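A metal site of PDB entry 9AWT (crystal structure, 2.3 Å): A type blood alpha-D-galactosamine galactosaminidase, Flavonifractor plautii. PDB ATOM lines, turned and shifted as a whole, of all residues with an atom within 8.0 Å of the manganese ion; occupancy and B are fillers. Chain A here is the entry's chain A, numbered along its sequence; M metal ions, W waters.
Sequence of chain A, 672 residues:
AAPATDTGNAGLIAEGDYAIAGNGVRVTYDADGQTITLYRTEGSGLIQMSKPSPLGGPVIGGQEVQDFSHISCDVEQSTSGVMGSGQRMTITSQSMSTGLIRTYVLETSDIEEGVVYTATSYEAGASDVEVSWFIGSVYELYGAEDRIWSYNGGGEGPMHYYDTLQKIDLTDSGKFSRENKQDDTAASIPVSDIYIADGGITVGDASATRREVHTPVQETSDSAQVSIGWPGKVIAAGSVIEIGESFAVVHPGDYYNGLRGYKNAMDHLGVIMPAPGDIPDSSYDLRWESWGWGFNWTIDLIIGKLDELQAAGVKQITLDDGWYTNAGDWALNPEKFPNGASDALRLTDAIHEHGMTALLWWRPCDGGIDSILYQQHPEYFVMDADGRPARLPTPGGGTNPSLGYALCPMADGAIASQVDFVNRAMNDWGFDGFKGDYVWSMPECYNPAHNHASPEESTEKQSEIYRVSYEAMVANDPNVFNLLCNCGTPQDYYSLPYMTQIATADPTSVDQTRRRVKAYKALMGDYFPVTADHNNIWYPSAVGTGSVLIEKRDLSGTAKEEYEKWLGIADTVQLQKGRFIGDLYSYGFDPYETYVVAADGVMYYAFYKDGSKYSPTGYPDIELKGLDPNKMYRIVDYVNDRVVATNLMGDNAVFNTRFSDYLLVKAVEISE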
ATOM      1  N   ASP A 146      17.394 -32.006  26.682  1.00  0.00           N
ATOM      2  CA  ASP A 146      17.857 -30.695  27.118  1.00  0.00           C
ATOM      3  C   ASP A 146      18.511 -30.772  28.492  1.00  0.00           C
ATOM      4  O   ASP A 146      19.324 -29.916  28.814  1.00  0.00           O
ATOM      5  CB  ASP A 146      16.752 -29.649  27.053  1.00  0.00           C
ATOM      6  CG  ASP A 146      15.541 -29.916  27.944  1.00  0.00           C
ATOM      7  OD1 ASP A 146      15.204 -31.100  28.083  1.00  0.00           O
ATOM      8  OD2 ASP A 146      14.975 -28.956  28.539  1.00  0.00           O
ATOM      9  N   LYS A 167      21.906 -30.917  38.331  1.00  0.00           N
ATOM     10  CA  LYS A 167      21.385 -30.890  36.973  1.00  0.00           C
ATOM     11  C   LYS A 167      22.542 -30.683  35.995  1.00  0.00           C
ATOM     12  O   LYS A 167      23.354 -29.780  36.156  1.00  0.00           O
ATOM     13  CB  LYS A 167      20.336 -29.790  36.814  1.00  0.00           C
ATOM     14  CG  LYS A 167      19.578 -29.846  35.484  1.00  0.00           C
ATOM     15  CD  LYS A 167      18.385 -28.904  35.378  1.00  0.00           C
ATOM     16  CE  LYS A 167      18.813 -27.507  35.107  1.00  0.00           C
ATOM     17  NZ  LYS A 167      17.664 -26.602  35.030  1.00  0.00           N
ATOM     18  N   ILE A 168      22.577 -31.509  34.946  1.00  0.00           N
ATOM     19  CA  ILE A 168      23.496 -31.352  33.835  1.00  0.00           C
ATOM     20  C   ILE A 168      22.714 -30.735  32.674  1.00  0.00           C
ATOM     21  O   ILE A 168      21.962 -31.418  32.011  1.00  0.00           O
ATOM     22  CB  ILE A 168      24.153 -32.694  33.463  1.00  0.00           C
ATOM     23  CG1 ILE A 168      24.832 -33.329  34.676  1.00  0.00           C
ATOM     24  CG2 ILE A 168      25.144 -32.523  32.299  1.00  0.00           C
ATOM     25  CD1 ILE A 168      25.253 -34.773  34.478  1.00  0.00           C
ATOM     26  N   ASP A 169      22.914 -29.433  32.474  1.00  0.00           N
ATOM     27  CA  ASP A 169      22.243 -28.674  31.441  1.00  0.00           C
ATOM     28  C   ASP A 169      23.032 -28.840  30.134  1.00  0.00           C
ATOM     29  O   ASP A 169      24.211 -28.542  30.068  1.00  0.00           O
ATOM     30  CB  ASP A 169      22.130 -27.213  31.868  1.00  0.00           C
ATOM     31  CG  ASP A 169      21.287 -26.292  30.981  1.00  0.00           C
ATOM     32  OD1 ASP A 169      20.951 -26.670  29.812  1.00  0.00           O
ATOM     33  OD2 ASP A 169      20.961 -25.213  31.459  1.00  0.00           O
ATOM     34  N   LEU A 170      22.328 -29.279  29.087  1.00  0.00           N
ATOM     35  CA  LEU A 170      22.916 -29.490  27.769  1.00  0.00           C
ATOM     36  C   LEU A 170      22.733 -28.286  26.839  1.00  0.00           C
ATOM     37  O   LEU A 170      23.118 -28.375  25.677  1.00  0.00           O
ATOM     38  CB  LEU A 170      22.311 -30.772  27.189  1.00  0.00           C
ATOM     39  CG  LEU A 170      22.434 -32.016  28.091  1.00  0.00           C
ATOM     40  CD1 LEU A 170      21.608 -33.206  27.643  1.00  0.00           C
ATOM     41  CD2 LEU A 170      23.876 -32.465  28.271  1.00  0.00           C
ATOM     42  N   THR A 171      22.155 -27.176  27.328  1.00  0.00           N
ATOM     43  CA  THR A 171      21.859 -26.032  26.469  1.00  0.00           C
ATOM     44  C   THR A 171      22.741 -24.832  26.795  1.00  0.00           C
ATOM     45  O   THR A 171      22.622 -23.792  26.170  1.00  0.00           O
ATOM     46  CB  THR A 171      20.374 -25.636  26.534  1.00  0.00           C
ATOM     47  OG1 THR A 171      20.105 -25.106  27.837  1.00  0.00           O
ATOM     48  CG2 THR A 171      19.437 -26.814  26.276  1.00  0.00           C
ATOM     49  N   ASP A 172      23.608 -24.953  27.797  1.00  0.00           N
ATOM     50  CA  ASP A 172      24.374 -23.830  28.371  1.00  0.00           C
ATOM     51  C   ASP A 172      25.800 -23.862  27.816  1.00  0.00           C
ATOM     52  O   ASP A 172      26.115 -24.673  26.958  1.00  0.00           O
ATOM     53  CB  ASP A 172      24.318 -23.838  29.899  1.00  0.00           C
ATOM     54  CG  ASP A 172      25.031 -25.006  30.565  1.00  0.00           C
ATOM     55  OD1 ASP A 172      25.493 -25.896  29.845  1.00  0.00           O
ATOM     56  OD2 ASP A 172      25.141 -25.028  31.825  1.00  0.00           O
ATOM     57  N   SER A 173      26.681 -23.007  28.304  1.00  0.00           N
ATOM     58  CA  SER A 173      28.081 -23.000  27.898  1.00  0.00           C
ATOM     59  C   SER A 173      28.920 -24.034  28.667  1.00  0.00           C
ATOM     60  O   SER A 173      29.869 -24.595  28.134  1.00  0.00           O
ATOM     61  CB  SER A 173      28.657 -21.615  28.030  1.00  0.00           C
ATOM     62  OG  SER A 173      30.059 -21.603  27.818  1.00  0.00           O
ATOM     63  N   GLY A 174      28.587 -24.326  29.922  1.00  0.00           N
ATOM     64  CA  GLY A 174      29.453 -25.137  30.784  1.00  0.00           C
ATOM     65  C   GLY A 174      29.433 -26.631  30.468  1.00  0.00           C
ATOM     66  O   GLY A 174      28.546 -27.129  29.776  1.00  0.00           O
ATOM     67  N   LYS A 175      30.454 -27.346  30.971  1.00  0.00           N
ATOM     68  CA  LYS A 175      30.566 -28.787  30.863  1.00  0.00           C
ATOM     69  C   LYS A 175      30.769 -29.358  32.273  1.00  0.00           C
ATOM     70  O   LYS A 175      31.810 -29.145  32.873  1.00  0.00           O
ATOM     71  CB  LYS A 175      31.735 -29.276  29.995  1.00  0.00           C
ATOM     72  CG  LYS A 175      31.651 -29.023  28.493  1.00  0.00           C
ATOM     73  CD  LYS A 175      30.431 -29.622  27.771  1.00  0.00           C
ATOM     74  CE  LYS A 175      30.411 -29.345  26.268  1.00  0.00           C
ATOM     75  NZ  LYS A 175      29.693 -30.390  25.513  1.00  0.00           N
ATOM     76  N   PHE A 176      29.762 -30.095  32.758  1.00  0.00           N
ATOM     77  CA  PHE A 176      29.781 -30.675  34.079  1.00  0.00           C
ATOM     78  C   PHE A 176      30.828 -31.799  34.190  1.00  0.00           C
ATOM     79  O   PHE A 176      30.853 -32.704  33.357  1.00  0.00           O
ATOM     80  CB  PHE A 176      28.378 -31.190  34.416  1.00  0.00           C
ATOM     81  CG  PHE A 176      28.238 -31.719  35.836  1.00  0.00           C
ATOM     82  CD1 PHE A 176      28.622 -33.007  36.167  1.00  0.00           C
ATOM     83  CD2 PHE A 176      27.716 -30.915  36.827  1.00  0.00           C
ATOM     84  CE1 PHE A 176      28.494 -33.472  37.480  1.00  0.00           C
ATOM     85  CE2 PHE A 176      27.577 -31.372  38.135  1.00  0.00           C
ATOM     86  CZ  PHE A 176      27.958 -32.661  38.452  1.00  0.00           C
ATOM     87  N   GLU A 219      29.685 -34.641  31.607  1.00  0.00           N
ATOM     88  CA  GLU A 219      28.900 -34.216  30.449  1.00  0.00           C
ATOM     89  C   GLU A 219      29.677 -34.500  29.173  1.00  0.00           C
ATOM     90  O   GLU A 219      30.894 -34.323  29.140  1.00  0.00           O
ATOM     91  CB  GLU A 219      28.588 -32.713  30.562  1.00  0.00           C
ATOM     92  CG  GLU A 219      27.662 -32.175  29.474  1.00  0.00           C
ATOM     93  CD  GLU A 219      27.212 -30.728  29.679  1.00  0.00           C
ATOM     94  OE1 GLU A 219      26.672 -30.159  28.698  1.00  0.00           O
ATOM     95  OE2 GLU A 219      27.419 -30.189  30.811  1.00  0.00           O
ATOM     96  N   THR A 220      28.952 -34.951  28.130  1.00  0.00           N
ATOM     97  CA  THR A 220      29.560 -35.205  26.824  1.00  0.00           C
ATOM     98  C   THR A 220      29.035 -34.161  25.840  1.00  0.00           C
ATOM     99  O   THR A 220      28.430 -33.182  26.254  1.00  0.00           O
ATOM    100  CB  THR A 220      29.255 -36.639  26.402  1.00  0.00           C
ATOM    101  OG1 THR A 220      27.862 -36.739  26.123  1.00  0.00           O
ATOM    102  CG2 THR A 220      29.588 -37.658  27.479  1.00  0.00           C
ATOM    103  N   SER A 221      29.225 -34.388  24.539  1.00  0.00           N
ATOM    104  CA  SER A 221      28.851 -33.427  23.525  1.00  0.00           C
ATOM    105  C   SER A 221      27.331 -33.243  23.456  1.00  0.00           C
ATOM    106  O   SER A 221      26.883 -32.115  23.219  1.00  0.00           O
ATOM    107  CB  SER A 221      29.430 -33.774  22.166  1.00  0.00           C
ATOM    108  OG  SER A 221      28.882 -34.998  21.686  1.00  0.00           O
ATOM    109  N   SER A 223      25.191 -35.437  25.749  1.00  0.00           N
ATOM    110  CA  SER A 223      24.649 -36.267  26.801  1.00  0.00           C
ATOM    111  C   SER A 223      25.566 -36.242  28.024  1.00  0.00           C
ATOM    112  O   SER A 223      26.318 -35.270  28.216  1.00  0.00           O
ATOM    113  CB  SER A 223      24.411 -37.678  26.254  1.00  0.00           C
ATOM    114  OG  SER A 223      23.788 -38.516  27.216  1.00  0.00           O
HETATM  115 MN    MN M   1      26.449 -27.983  30.015  1.00  0.00          MN
HETATM  116  O   HOH W   1      26.668 -27.302  32.653  1.00  0.00           O
HETATM  117  O   HOH W   2      26.132 -27.374  27.605  1.00  0.00           O
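The side-chain carboxylate (OD1) of Asp 169 lies within hydrogen-bond range of the side-chain hydroxyl (OG1) of Thr 171 (2.7 Å). N of Glu 219 lies within hydrogen-bond range of O of Phe 176, 2.9 Å away.
Four residues have an atom within 4 Å of the manganese ion: Asp 169, Asp 172, Gly 174 and Glu 219.
The manganese ion is bound by the backbone carbonyl oxygen (O) of Gly 174 (2.3 Å), the side-chain carboxylate (OD1) of Asp 172 (2.3 Å), the backbone carbonyl oxygen (O) of Asp 169 (2.3 Å), water W2 (2.5 Å), the side-chain carboxylate (OE2) of Glu 219 (2.5 Å) and the side-chain carboxylate (OE1) of Glu 219 (2.6 Å). The manganese ion has six donor atoms within binding distance. Slightly farther from the manganese ion lies water W1 (2.7 Å).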
